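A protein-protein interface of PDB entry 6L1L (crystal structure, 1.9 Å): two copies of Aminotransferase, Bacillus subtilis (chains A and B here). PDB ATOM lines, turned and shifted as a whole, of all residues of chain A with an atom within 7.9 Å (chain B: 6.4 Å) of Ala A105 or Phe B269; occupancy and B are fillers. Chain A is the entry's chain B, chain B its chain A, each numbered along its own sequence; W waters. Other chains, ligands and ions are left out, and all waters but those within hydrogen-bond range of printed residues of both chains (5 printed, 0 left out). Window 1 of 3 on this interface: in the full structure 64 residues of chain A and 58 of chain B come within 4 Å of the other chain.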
ATOM      1  N   ARG A  14     -30.696  -1.509  12.283  1.00  0.00           N
ATOM      2  CA  ARG A  14     -31.360  -2.460  11.400  1.00  0.00           C
ATOM      3  C   ARG A  14     -31.704  -3.642  12.291  1.00  0.00           C
ATOM      4  O   ARG A  14     -30.818  -4.226  12.928  1.00  0.00           O
ATOM      5  CB  ARG A  14     -30.476  -2.872  10.220  1.00  0.00           C
ATOM      6  CG  ARG A  14     -31.051  -4.018   9.374  1.00  0.00           C
ATOM      7  CD  ARG A  14     -32.140  -3.548   8.439  1.00  0.00           C
ATOM      8  N   LEU A  99     -31.240  -0.319 -13.355  1.00  0.00           N
ATOM      9  CA  LEU A  99     -30.836  -1.528 -12.568  1.00  0.00           C
ATOM     10  C   LEU A  99     -30.251  -1.171 -11.207  1.00  0.00           C
ATOM     11  O   LEU A  99     -29.513  -0.192 -11.091  1.00  0.00           O
ATOM     12  CB  LEU A  99     -29.793  -2.297 -13.336  1.00  0.00           C
ATOM     13  CG  LEU A  99     -30.080  -2.687 -14.773  1.00  0.00           C
ATOM     14  CD1 LEU A  99     -28.840  -3.386 -15.299  1.00  0.00           C
ATOM     15  CD2 LEU A  99     -31.291  -3.570 -14.907  1.00  0.00           C
ATOM     16  N   PHE A 100     -30.540  -2.012 -10.209  1.00  0.00           N
ATOM     17  CA  PHE A 100     -30.051  -1.858  -8.842  1.00  0.00           C
ATOM     18  C   PHE A 100     -29.484  -3.163  -8.304  1.00  0.00           C
ATOM     19  O   PHE A 100     -29.974  -4.248  -8.646  1.00  0.00           O
ATOM     20  CB  PHE A 100     -31.148  -1.466  -7.890  1.00  0.00           C
ATOM     21  CG  PHE A 100     -31.868  -0.190  -8.250  1.00  0.00           C
ATOM     22  CD1 PHE A 100     -31.217   1.024  -8.226  1.00  0.00           C
ATOM     23  CD2 PHE A 100     -33.235  -0.219  -8.540  1.00  0.00           C
ATOM     24  CE1 PHE A 100     -31.909   2.205  -8.524  1.00  0.00           C
ATOM     25  CE2 PHE A 100     -33.928   0.958  -8.816  1.00  0.00           C
ATOM     26  CZ  PHE A 100     -33.268   2.158  -8.828  1.00  0.00           C
ATOM     27  N   GLY A 101     -28.484  -3.033  -7.434  1.00  0.00           N
ATOM     28  CA  GLY A 101     -28.022  -4.154  -6.597  1.00  0.00           C
ATOM     29  C   GLY A 101     -29.008  -4.481  -5.455  1.00  0.00           C
ATOM     30  O   GLY A 101     -28.694  -4.334  -4.266  1.00  0.00           O
ATOM     31  N   GLY A 102     -30.186  -4.965  -5.811  1.00  0.00           N
ATOM     32  CA  GLY A 102     -31.254  -5.236  -4.882  1.00  0.00           C
ATOM     33  C   GLY A 102     -32.233  -4.090  -4.600  1.00  0.00           C
ATOM     34  O   GLY A 102     -31.928  -2.926  -4.765  1.00  0.00           O
ATOM     35  N   GLY A 103     -33.443  -4.462  -4.198  1.00  0.00           N
ATOM     36  CA  GLY A 103     -34.505  -3.526  -3.941  1.00  0.00           C
ATOM     37  C   GLY A 103     -34.214  -2.582  -2.820  1.00  0.00           C
ATOM     38  O   GLY A 103     -34.613  -1.424  -2.836  1.00  0.00           O
ATOM     39  N   LYS A 104     -33.488  -3.062  -1.821  1.00  0.00           N
ATOM     40  CA  LYS A 104     -33.095  -2.206  -0.732  1.00  0.00           C
ATOM     41  C   LYS A 104     -32.181  -1.058  -1.190  1.00  0.00           C
ATOM     42  O   LYS A 104     -32.298   0.070  -0.712  1.00  0.00           O
ATOM     43  CB  LYS A 104     -32.425  -3.046   0.356  1.00  0.00           C
ATOM     44  CG  LYS A 104     -31.902  -2.246   1.475  1.00  0.00           C
ATOM     45  CD  LYS A 104     -32.301  -2.757   2.822  1.00  0.00           C
ATOM     46  CE  LYS A 104     -31.670  -4.049   3.147  1.00  0.00           C
ATOM     47  NZ  LYS A 104     -32.594  -5.170   2.800  1.00  0.00           N
ATOM     48  N   ALA A 105     -31.324  -1.329  -2.147  1.00  0.00           N
ATOM     49  CA  ALA A 105     -30.429  -0.309  -2.709  1.00  0.00           C
ATOM     50  C   ALA A 105     -31.262   0.657  -3.583  1.00  0.00           C
ATOM     51  O   ALA A 105     -31.027   1.868  -3.579  1.00  0.00           O
ATOM     52  CB  ALA A 105     -29.356  -0.938  -3.546  1.00  0.00           C
ATOM     53  N   GLY A 106     -32.256   0.090  -4.265  1.00  0.00           N
ATOM     54  CA  GLY A 106     -33.150   0.827  -5.140  1.00  0.00           C
ATOM     55  C   GLY A 106     -33.830   1.912  -4.352  1.00  0.00           C
ATOM     56  O   GLY A 106     -33.839   3.075  -4.773  1.00  0.00           O
ATOM     57  N   LEU A 107     -34.408   1.497  -3.217  1.00  0.00           N
ATOM     58  CA  LEU A 107     -35.094   2.390  -2.310  1.00  0.00           C
ATOM     59  C   LEU A 107     -34.236   3.520  -1.864  1.00  0.00           C
ATOM     60  O   LEU A 107     -34.712   4.658  -1.854  1.00  0.00           O
ATOM     61  CB  LEU A 107     -35.662   1.636  -1.116  1.00  0.00           C
ATOM     62  CG  LEU A 107     -36.853   0.727  -1.396  1.00  0.00           C
ATOM     63  CD1 LEU A 107     -37.127  -0.081  -0.134  1.00  0.00           C
ATOM     64  CD2 LEU A 107     -38.090   1.489  -1.887  1.00  0.00           C
ATOM     65  N   TYR A 108     -33.010   3.230  -1.409  1.00  0.00           N
ATOM     66  CA  TYR A 108     -32.069   4.270  -1.028  1.00  0.00           C
ATOM     67  C   TYR A 108     -31.800   5.262  -2.209  1.00  0.00           C
ATOM     68  O   TYR A 108     -31.912   6.500  -2.087  1.00  0.00           O
ATOM     69  CB  TYR A 108     -30.748   3.667  -0.556  1.00  0.00           C
ATOM     70  CG  TYR A 108     -29.714   4.717  -0.288  1.00  0.00           C
ATOM     71  CD1 TYR A 108     -29.761   5.459   0.855  1.00  0.00           C
ATOM     72  CD2 TYR A 108     -28.723   5.016  -1.224  1.00  0.00           C
ATOM     73  CE1 TYR A 108     -28.835   6.449   1.108  1.00  0.00           C
ATOM     74  CE2 TYR A 108     -27.798   6.005  -0.980  1.00  0.00           C
ATOM     75  CZ  TYR A 108     -27.848   6.702   0.207  1.00  0.00           C
ATOM     76  OH  TYR A 108     -26.947   7.678   0.460  1.00  0.00           O
ATOM     77  N   VAL A 109     -31.491   4.712  -3.365  1.00  0.00           N
ATOM     78  CA  VAL A 109     -31.185   5.559  -4.537  1.00  0.00           C
ATOM     79  C   VAL A 109     -32.382   6.455  -4.964  1.00  0.00           C
ATOM     80  O   VAL A 109     -32.192   7.624  -5.257  1.00  0.00           O
ATOM     81  CB  VAL A 109     -30.668   4.725  -5.710  1.00  0.00           C
ATOM     82  CG1 VAL A 109     -30.412   5.595  -6.922  1.00  0.00           C
ATOM     83  CG2 VAL A 109     -29.365   4.037  -5.339  1.00  0.00           C
ATOM     84  N   LEU A 110     -33.588   5.896  -4.986  1.00  0.00           N
ATOM     85  CA  LEU A 110     -34.783   6.604  -5.359  1.00  0.00           C
ATOM     86  C   LEU A 110     -35.088   7.689  -4.362  1.00  0.00           C
ATOM     87  O   LEU A 110     -35.465   8.796  -4.757  1.00  0.00           O
ATOM     88  CB  LEU A 110     -35.972   5.676  -5.444  1.00  0.00           C
ATOM     89  CG  LEU A 110     -36.023   4.837  -6.714  1.00  0.00           C
ATOM     90  CD1 LEU A 110     -36.969   3.641  -6.526  1.00  0.00           C
ATOM     91  CD2 LEU A 110     -36.437   5.686  -7.914  1.00  0.00           C
ATOM     92  N   THR A 111     -34.910   7.391  -3.075  1.00  0.00           N
ATOM     93  CA  THR A 111     -35.082   8.384  -2.058  1.00  0.00           C
ATOM     94  C   THR A 111     -34.116   9.557  -2.238  1.00  0.00           C
ATOM     95  O   THR A 111     -34.537  10.722  -2.137  1.00  0.00           O
ATOM     96  CB  THR A 111     -34.936   7.759  -0.662  1.00  0.00           C
ATOM     97  OG1 THR A 111     -36.101   6.970  -0.402  1.00  0.00           O
ATOM     98  CG2 THR A 111     -34.879   8.814   0.370  1.00  0.00           C
ATOM     99  N   GLN A 112     -32.836   9.256  -2.488  1.00  0.00           N
ATOM    100  CA  GLN A 112     -31.821  10.296  -2.635  1.00  0.00           C
ATOM    101  C   GLN A 112     -32.016  11.112  -3.913  1.00  0.00           C
ATOM    102  O   GLN A 112     -31.637  12.278  -3.960  1.00  0.00           O
ATOM    103  CB  GLN A 112     -30.407   9.717  -2.640  1.00  0.00           C
ATOM    104  CG  GLN A 112     -29.992   8.918  -1.391  1.00  0.00           C
ATOM    105  CD  GLN A 112     -29.898   9.755  -0.161  1.00  0.00           C
ATOM    106  OE1 GLN A 112     -30.589   9.498   0.833  1.00  0.00           O
ATOM    107  NE2 GLN A 112     -29.068  10.773  -0.208  1.00  0.00           N
ATOM    108  N   TYR A 128     -42.578  -1.336   5.356  1.00  0.00           N
ATOM    109  CA  TYR A 128     -41.184  -1.765   5.294  1.00  0.00           C
ATOM    110  C   TYR A 128     -40.275  -0.721   5.978  1.00  0.00           C
ATOM    111  O   TYR A 128     -40.357   0.435   5.666  1.00  0.00           O
ATOM    112  CB  TYR A 128     -40.797  -1.981   3.804  1.00  0.00           C
ATOM    113  CG  TYR A 128     -39.449  -2.598   3.559  1.00  0.00           C
ATOM    114  CD1 TYR A 128     -39.055  -3.776   4.221  1.00  0.00           C
ATOM    115  CD2 TYR A 128     -38.567  -2.044   2.652  1.00  0.00           C
ATOM    116  CE1 TYR A 128     -37.814  -4.343   3.998  1.00  0.00           C
ATOM    117  CE2 TYR A 128     -37.339  -2.618   2.403  1.00  0.00           C
ATOM    118  CZ  TYR A 128     -36.960  -3.762   3.083  1.00  0.00           C
ATOM    119  OH  TYR A 128     -35.724  -4.312   2.863  1.00  0.00           O
ATOM    120  N   GLU A 130     -37.256   0.160   5.721  1.00  0.00           N
ATOM    121  CA  GLU A 130     -36.284   0.910   4.961  1.00  0.00           C
ATOM    122  C   GLU A 130     -36.858   2.192   4.340  1.00  0.00           C
ATOM    123  O   GLU A 130     -36.094   3.108   4.039  1.00  0.00           O
ATOM    124  CB  GLU A 130     -35.606   0.025   3.913  1.00  0.00           C
ATOM    125  CG  GLU A 130     -34.932  -1.215   4.521  1.00  0.00           C
ATOM    126  CD  GLU A 130     -34.042  -0.950   5.728  1.00  0.00           C
ATOM    127  OE1 GLU A 130     -33.351   0.093   5.780  1.00  0.00           O
ATOM    128  OE2 GLU A 130     -34.012  -1.809   6.644  1.00  0.00           O
ATOM    129  N   LEU A 234     -40.716  -0.547  -8.429  1.00  0.00           N
ATOM    130  CA  LEU A 234     -39.558  -1.338  -8.041  1.00  0.00           C
ATOM    131  C   LEU A 234     -39.857  -2.843  -8.022  1.00  0.00           C
ATOM    132  O   LEU A 234     -40.728  -3.300  -7.244  1.00  0.00           O
ATOM    133  CB  LEU A 234     -39.073  -0.924  -6.657  1.00  0.00           C
ATOM    134  CG  LEU A 234     -37.775  -1.520  -6.183  1.00  0.00           C
ATOM    135  CD1 LEU A 234     -36.630  -1.203  -7.151  1.00  0.00           C
ATOM    136  CD2 LEU A 234     -37.445  -1.007  -4.788  1.00  0.00           C
ATOM    137  N   ARG A 247     -28.676 -10.266  -5.123  1.00  0.00           N
ATOM    138  CA  ARG A 247     -28.723  -8.784  -4.989  1.00  0.00           C
ATOM    139  C   ARG A 247     -29.038  -8.081  -6.312  1.00  0.00           C
ATOM    140  O   ARG A 247     -28.194  -7.334  -6.866  1.00  0.00           O
ATOM    141  CB  ARG A 247     -27.453  -8.248  -4.355  1.00  0.00           C
ATOM    142  CG  ARG A 247     -27.037  -8.864  -3.008  1.00  0.00           C
ATOM    143  CD  ARG A 247     -28.117  -9.068  -1.935  1.00  0.00           C
ATOM    144  NE  ARG A 247     -28.876  -7.815  -1.658  1.00  0.00           N
ATOM    145  CZ  ARG A 247     -30.207  -7.715  -1.594  1.00  0.00           C
ATOM    146  NH1 ARG A 247     -30.980  -8.762  -1.770  1.00  0.00           N
ATOM    147  NH2 ARG A 247     -30.775  -6.526  -1.332  1.00  0.00           N
ATOM    148  N   ALA A 249     -32.256  -6.140  -8.803  1.00  0.00           N
ATOM    149  CA  ALA A 249     -33.551  -5.478  -8.860  1.00  0.00           C
ATOM    150  C   ALA A 249     -33.577  -4.465  -9.979  1.00  0.00           C
ATOM    151  O   ALA A 249     -32.548  -4.140 -10.593  1.00  0.00           O
ATOM    152  CB  ALA A 249     -33.847  -4.792  -7.545  1.00  0.00           C
ATOM    153  N   PHE A 264     -27.227   9.588 -10.779  1.00  0.00           N
ATOM    154  CA  PHE A 264     -26.634   9.181  -9.487  1.00  0.00           C
ATOM    155  C   PHE A 264     -25.669   7.998  -9.617  1.00  0.00           C
ATOM    156  O   PHE A 264     -24.531   8.051  -9.156  1.00  0.00           O
ATOM    157  CB  PHE A 264     -27.737   8.811  -8.520  1.00  0.00           C
ATOM    158  CG  PHE A 264     -27.249   8.364  -7.165  1.00  0.00           C
ATOM    159  CD1 PHE A 264     -27.271   9.233  -6.089  1.00  0.00           C
ATOM    160  CD2 PHE A 264     -26.856   7.047  -6.949  1.00  0.00           C
ATOM    161  CE1 PHE A 264     -26.860   8.818  -4.837  1.00  0.00           C
ATOM    162  CE2 PHE A 264     -26.418   6.621  -5.701  1.00  0.00           C
ATOM    163  CZ  PHE A 264     -26.426   7.518  -4.642  1.00  0.00           C
ATOM    164  N   GLN A 265     -26.160   6.929 -10.220  1.00  0.00           N
ATOM    165  CA  GLN A 265     -25.463   5.660 -10.213  1.00  0.00           C
ATOM    166  C   GLN A 265     -24.240   5.616 -11.101  1.00  0.00           C
ATOM    167  O   GLN A 265     -23.333   4.816 -10.843  1.00  0.00           O
ATOM    168  CB  GLN A 265     -26.420   4.518 -10.541  1.00  0.00           C
ATOM    169  CG  GLN A 265     -27.451   4.372  -9.456  1.00  0.00           C
ATOM    170  CD  GLN A 265     -28.261   3.088  -9.479  1.00  0.00           C
ATOM    171  OE1 GLN A 265     -28.506   2.493  -8.417  1.00  0.00           O
ATOM    172  NE2 GLN A 265     -28.712   2.666 -10.652  1.00  0.00           N
ATOM    173  N   VAL A 268     -21.568   6.243  -8.590  1.00  0.00           N
ATOM    174  CA  VAL A 268     -21.437   5.329  -7.441  1.00  0.00           C
ATOM    175  C   VAL A 268     -21.291   3.840  -7.863  1.00  0.00           C
ATOM    176  O   VAL A 268     -20.786   3.072  -7.084  1.00  0.00           O
ATOM    177  CB  VAL A 268     -22.592   5.527  -6.458  1.00  0.00           C
ATOM    178  CG1 VAL A 268     -22.371   4.778  -5.160  1.00  0.00           C
ATOM    179  CG2 VAL A 268     -22.727   7.011  -6.134  1.00  0.00           C
ATOM    180  N   PHE A 269     -21.605   3.486  -9.123  1.00  0.00           N
ATOM    181  CA  PHE A 269     -21.740   2.060  -9.563  1.00  0.00           C
ATOM    182  C   PHE A 269     -21.066   1.555 -10.861  1.00  0.00           C
ATOM    183  O   PHE A 269     -20.095   0.750 -10.829  1.00  0.00           O
ATOM    184  CB  PHE A 269     -23.225   1.649  -9.521  1.00  0.00           C
ATOM    185  CG  PHE A 269     -23.776   1.606  -8.107  1.00  0.00           C
ATOM    186  CD1 PHE A 269     -23.017   1.071  -7.053  1.00  0.00           C
ATOM    187  CD2 PHE A 269     -25.029   2.074  -7.814  1.00  0.00           C
ATOM    188  CE1 PHE A 269     -23.502   1.057  -5.745  1.00  0.00           C
ATOM    189  CE2 PHE A 269     -25.525   2.052  -6.518  1.00  0.00           C
ATOM    190  CZ  PHE A 269     -24.756   1.561  -5.484  1.00  0.00           C
ATOM    191  N   PHE B  69     -25.205  -9.717   6.592  1.00  0.00           N
ATOM    192  CA  PHE B  69     -25.230  -8.317   6.110  1.00  0.00           C
ATOM    193  C   PHE B  69     -23.836  -7.734   5.864  1.00  0.00           C
ATOM    194  O   PHE B  69     -23.644  -6.912   4.987  1.00  0.00           O
ATOM    195  CB  PHE B  69     -25.938  -7.390   7.125  1.00  0.00           C
ATOM    196  CG  PHE B  69     -27.418  -7.586   7.185  1.00  0.00           C
ATOM    197  CD1 PHE B  69     -28.264  -6.777   6.444  1.00  0.00           C
ATOM    198  CD2 PHE B  69     -27.980  -8.592   7.991  1.00  0.00           C
ATOM    199  CE1 PHE B  69     -29.646  -6.967   6.478  1.00  0.00           C
ATOM    200  CE2 PHE B  69     -29.368  -8.783   8.022  1.00  0.00           C
ATOM    201  CZ  PHE B  69     -30.193  -7.963   7.249  1.00  0.00           C
ATOM    202  N   GLY B 101     -19.306  -3.023  -3.125  1.00  0.00           N
ATOM    203  CA  GLY B 101     -19.489  -3.362  -4.543  1.00  0.00           C
ATOM    204  C   GLY B 101     -18.607  -2.520  -5.448  1.00  0.00           C
ATOM    205  O   GLY B 101     -19.095  -1.761  -6.232  1.00  0.00           O
ATOM    206  N   ALA B 105     -18.140   2.619  -5.168  1.00  0.00           N
ATOM    207  CA  ALA B 105     -19.174   2.596  -4.134  1.00  0.00           C
ATOM    208  C   ALA B 105     -18.528   2.800  -2.707  1.00  0.00           C
ATOM    209  O   ALA B 105     -19.123   3.367  -1.797  1.00  0.00           O
ATOM    210  CB  ALA B 105     -19.980   1.336  -4.222  1.00  0.00           C
ATOM    211  N   VAL B 109     -19.613   5.501   0.062  1.00  0.00           N
ATOM    212  CA  VAL B 109     -20.040   5.136   1.401  1.00  0.00           C
ATOM    213  C   VAL B 109     -19.158   5.786   2.476  1.00  0.00           C
ATOM    214  O   VAL B 109     -19.701   6.265   3.505  1.00  0.00           O
ATOM    215  CB  VAL B 109     -20.099   3.623   1.537  1.00  0.00           C
ATOM    216  CG1 VAL B 109     -20.228   3.182   2.989  1.00  0.00           C
ATOM    217  CG2 VAL B 109     -21.250   3.106   0.726  1.00  0.00           C
ATOM    218  N   PHE B 264     -24.281   2.136   8.036  1.00  0.00           N
ATOM    219  CA  PHE B 264     -24.826   2.646   6.772  1.00  0.00           C
ATOM    220  C   PHE B 264     -25.263   1.502   5.898  1.00  0.00           C
ATOM    221  O   PHE B 264     -26.400   1.401   5.481  1.00  0.00           O
ATOM    222  CB  PHE B 264     -23.776   3.469   6.024  1.00  0.00           C
ATOM    223  CG  PHE B 264     -24.302   4.138   4.757  1.00  0.00           C
ATOM    224  CD1 PHE B 264     -24.704   5.457   4.766  1.00  0.00           C
ATOM    225  CD2 PHE B 264     -24.368   3.432   3.547  1.00  0.00           C
ATOM    226  CE1 PHE B 264     -25.182   6.068   3.617  1.00  0.00           C
ATOM    227  CE2 PHE B 264     -24.841   4.031   2.402  1.00  0.00           C
ATOM    228  CZ  PHE B 264     -25.248   5.356   2.431  1.00  0.00           C
ATOM    229  N   GLN B 265     -24.344   0.584   5.631  1.00  0.00           N
ATOM    230  CA  GLN B 265     -24.656  -0.471   4.678  1.00  0.00           C
ATOM    231  C   GLN B 265     -25.687  -1.457   5.107  1.00  0.00           C
ATOM    232  O   GLN B 265     -26.298  -2.072   4.262  1.00  0.00           O
ATOM    233  CB  GLN B 265     -23.371  -1.152   4.230  1.00  0.00           C
ATOM    234  CG  GLN B 265     -22.405  -0.178   3.594  1.00  0.00           C
ATOM    235  CD  GLN B 265     -21.343  -0.916   2.772  1.00  0.00           C
ATOM    236  OE1 GLN B 265     -20.522  -1.667   3.309  1.00  0.00           O
ATOM    237  NE2 GLN B 265     -21.345  -0.688   1.495  1.00  0.00           N
ATOM    238  N   ASP B 266     -25.923  -1.606   6.417  1.00  0.00           N
ATOM    239  CA  ASP B 266     -27.029  -2.444   6.921  1.00  0.00           C
ATOM    240  C   ASP B 266     -28.390  -2.022   6.355  1.00  0.00           C
ATOM    241  O   ASP B 266     -29.263  -2.855   6.145  1.00  0.00           O
ATOM    242  CB  ASP B 266     -27.088  -2.411   8.452  1.00  0.00           C
ATOM    243  CG  ASP B 266     -26.129  -3.361   9.131  1.00  0.00           C
ATOM    244  OD1 ASP B 266     -25.308  -4.044   8.469  1.00  0.00           O
ATOM    245  OD2 ASP B 266     -26.206  -3.437  10.392  1.00  0.00           O
ATOM    246  N   HIS B 267     -28.567  -0.714   6.127  1.00  0.00           N
ATOM    247  CA  HIS B 267     -29.805  -0.194   5.583  1.00  0.00           C
ATOM    248  C   HIS B 267     -29.867  -0.198   4.066  1.00  0.00           C
ATOM    249  O   HIS B 267     -30.939  -0.020   3.497  1.00  0.00           O
ATOM    250  CB  HIS B 267     -30.017   1.236   6.089  1.00  0.00           C
ATOM    251  CG  HIS B 267     -30.176   1.304   7.567  1.00  0.00           C
ATOM    252  ND1 HIS B 267     -31.368   1.026   8.203  1.00  0.00           N
ATOM    253  CD2 HIS B 267     -29.271   1.534   8.539  1.00  0.00           C
ATOM    254  CE1 HIS B 267     -31.192   1.115   9.509  1.00  0.00           C
ATOM    255  NE2 HIS B 267     -29.928   1.417   9.737  1.00  0.00           N
ATOM    256  N   VAL B 268     -28.728  -0.357   3.417  1.00  0.00           N
ATOM    257  CA  VAL B 268     -28.649  -0.146   1.983  1.00  0.00           C
ATOM    258  C   VAL B 268     -28.426  -1.476   1.216  1.00  0.00           C
ATOM    259  O   VAL B 268     -28.947  -1.648   0.121  1.00  0.00           O
ATOM    260  CB  VAL B 268     -27.563   0.872   1.645  1.00  0.00           C
ATOM    261  CG1 VAL B 268     -27.438   1.050   0.118  1.00  0.00           C
ATOM    262  CG2 VAL B 268     -27.907   2.206   2.286  1.00  0.00           C
ATOM    263  N   PHE B 269     -27.735  -2.410   1.855  1.00  0.00           N
ATOM    264  CA  PHE B 269     -27.395  -3.694   1.255  1.00  0.00           C
ATOM    265  C   PHE B 269     -27.607  -4.887   2.159  1.00  0.00           C
ATOM    266  O   PHE B 269     -27.951  -4.742   3.356  1.00  0.00           O
ATOM    267  CB  PHE B 269     -25.950  -3.651   0.847  1.00  0.00           C
ATOM    268  CG  PHE B 269     -25.617  -2.504  -0.049  1.00  0.00           C
ATOM    269  CD1 PHE B 269     -26.217  -2.384  -1.292  1.00  0.00           C
ATOM    270  CD2 PHE B 269     -24.690  -1.577   0.326  1.00  0.00           C
ATOM    271  CE1 PHE B 269     -25.887  -1.353  -2.144  1.00  0.00           C
ATOM    272  CE2 PHE B 269     -24.360  -0.541  -0.509  1.00  0.00           C
ATOM    273  CZ  PHE B 269     -24.955  -0.430  -1.748  1.00  0.00           C
ATOM    274  N   VAL B 270     -27.464  -6.077   1.553  1.00  0.00           N
ATOM    275  CA  VAL B 270     -27.431  -7.339   2.305  1.00  0.00           C
ATOM    276  C   VAL B 270     -26.239  -8.163   1.837  1.00  0.00           C
ATOM    277  O   VAL B 270     -26.380  -9.233   1.282  1.00  0.00           O
ATOM    278  CB  VAL B 270     -28.732  -8.157   2.182  1.00  0.00           C
ATOM    279  CG1 VAL B 270     -28.709  -9.314   3.187  1.00  0.00           C
ATOM    280  CG2 VAL B 270     -29.955  -7.277   2.420  1.00  0.00           C
ATOM    281  N   GLY B 271     -25.046  -7.632   2.095  1.00  0.00           N
ATOM    282  CA  GLY B 271     -23.831  -8.224   1.626  1.00  0.00           C
ATOM    283  C   GLY B 271     -23.808  -8.199   0.116  1.00  0.00           C
ATOM    284  O   GLY B 271     -24.108  -7.157  -0.482  1.00  0.00           O
ATOM    285  N   MET B 272     -23.442  -9.323  -0.477  1.00  0.00           N
ATOM    286  CA  MET B 272     -23.223  -9.450  -1.918  1.00  0.00           C
ATOM    287  C   MET B 272     -23.103 -10.952  -2.228  1.00  0.00           C
ATOM    288  O   MET B 272     -22.836 -11.744  -1.338  1.00  0.00           O
ATOM    289  CB  MET B 272     -21.966  -8.738  -2.343  1.00  0.00           C
ATOM    290  CG  MET B 272     -20.679  -9.330  -1.797  1.00  0.00           C
ATOM    291  SD  MET B 272     -19.231  -8.653  -2.587  1.00  0.00           S
ATOM    292  CE  MET B 272     -19.210  -7.020  -1.874  1.00  0.00           C
HETATM  293  O   HOH W   1     -26.802  -6.033  -1.452  1.00  0.00           O
HETATM  294  O   HOH W   2     -18.842   0.679  -7.441  1.00  0.00           O
HETATM  295  O   HOH W   3     -27.583  -1.753  11.918  1.00  0.00           O
HETATM  296  O   HOH W   4     -29.345  -3.707  -1.656  1.00  0.00           O
HETATM  297  O   HOH W   5     -33.022   0.908   1.641  1.00  0.00           O
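The backbone carbonyl oxygen (O) of Val B268 is in hydrogen-bond range of the backbone NH (N) of Ala A105, at 3.3 Å. A ring nitrogen (ND1) of His B267 lies within hydrogen-bond range of the side-chain carboxylate (OE1) of Glu A130 (3.3 Å). The backbone NH (N) of Ala B105 is in hydrogen-bond range of the backbone carbonyl oxygen (O) of Val A268, 3.3 Å away.
N of Gly A102 is in hydrogen-bond range of O of Arg A247 (3.3 Å). OH of Tyr A128 sits at hydrogen-bond distance from NZ of Lys A104 (3.2 Å).
Among the printed residues, merely in contact across the chains: Arg A14 with Asp B266 (3.7 Å), Arg A14 with His B267 (3.9 Å), Lys A104 with His B267 (3.1 Å), Lys A104 with Val B268 (3.3 Å), Lys A104 with Phe B269 (3.8 Å), Lys A104 with Val B270 (3.4 Å), Ala A105 with Phe B269 (3.8 Å), Tyr A108 with Phe B264 (3.5 Å), Arg A247 with Val B270 (3.7 Å) and Phe A269 with Ala B105 (3.8 Å).
Of the printed residues of chain B, Lys A104 touches His B267, Val B268, Phe B269 and Val B270. Of chain B, only Val B268 (3.3 Å) and Phe B269 (3.8 Å) come within 4 Å of Ala A105. Gln A112 touches none of the printed residues of chain B. Tyr A128 touches none of the printed residues of chain B. Printed residues of chain A within 4 Å of Phe B264: Tyr A108 (3.5 Å). Of the printed residues of chain A, Asp B266 touches Arg A14. Of the printed residues of chain A, Phe B269 touches Lys A104 (3.8 Å) and Ala A105 (3.8 Å). Of the printed residues of chain A, Val B270 touches Lys A104 (3.4 Å) and Arg A247 (3.7 Å). The nearest residue of chain A that does not touch Phe B269 is Phe A269 (4.2 Å). The nearest printed residue of chain A that does not touch Val B270 is Gly A101 (6.2 Å).
Hydrophobic or aromatic side chains of chain B that line the printed part of chain A: Ala B105, Phe B264, His B267, Phe B269 and Val B270. Of the 24 printed residues of chain A, 8 touch a printed residue of chain B. Hydrophobic or aromatic side chains of chain A within 4 Å of the printed part of chain B: Ala A105, Tyr A108 and Phe A269.
Ala A105 touches Val B268, and with the chains exchanged Val A268 touches Ala B105. Ala A105 touches Phe B269, and with the chains exchanged Phe A269 touches Ala B105. Of the 13 pairs that touch across the chains among the printed residues, 4 have their exchanged pair printed and touching as well.
Water W5 lies within hydrogen-bond range of the backbone carbonyl oxygen of Lys A104 (2.6 Å) and the backbone carbonyl oxygen of His B267 (2.9 Å). Water W3 lies within hydrogen-bond range of the side-chain carboxylate (OD2) of Asp B266 (2.7 Å) and the backbone NH (N) of Arg A14 (3.1 Å). Water W2 lies within hydrogen-bond range of the backbone carbonyl oxygen (O) of Gly B101 (2.7 Å), the backbone NH (N) of Ala B105 (3.1 Å) and the backbone carbonyl oxygen (O) of Val A268 (3.1 Å). Water W1 lies within hydrogen-bond range of the guanidinium group (NE) of Arg A247 (2.7 Å), the backbone carbonyl oxygen (O) of Gly B271 (3.1 Å) and the backbone NH (N) of Val B270 (3.1 Å). Water W4 lies within hydrogen-bond range of O of Val B268 (2.7 Å), O of Gly A101 (2.8 Å), N of Ala A105 (3.1 Å) and NH2 of Arg A247 (3.2 Å).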
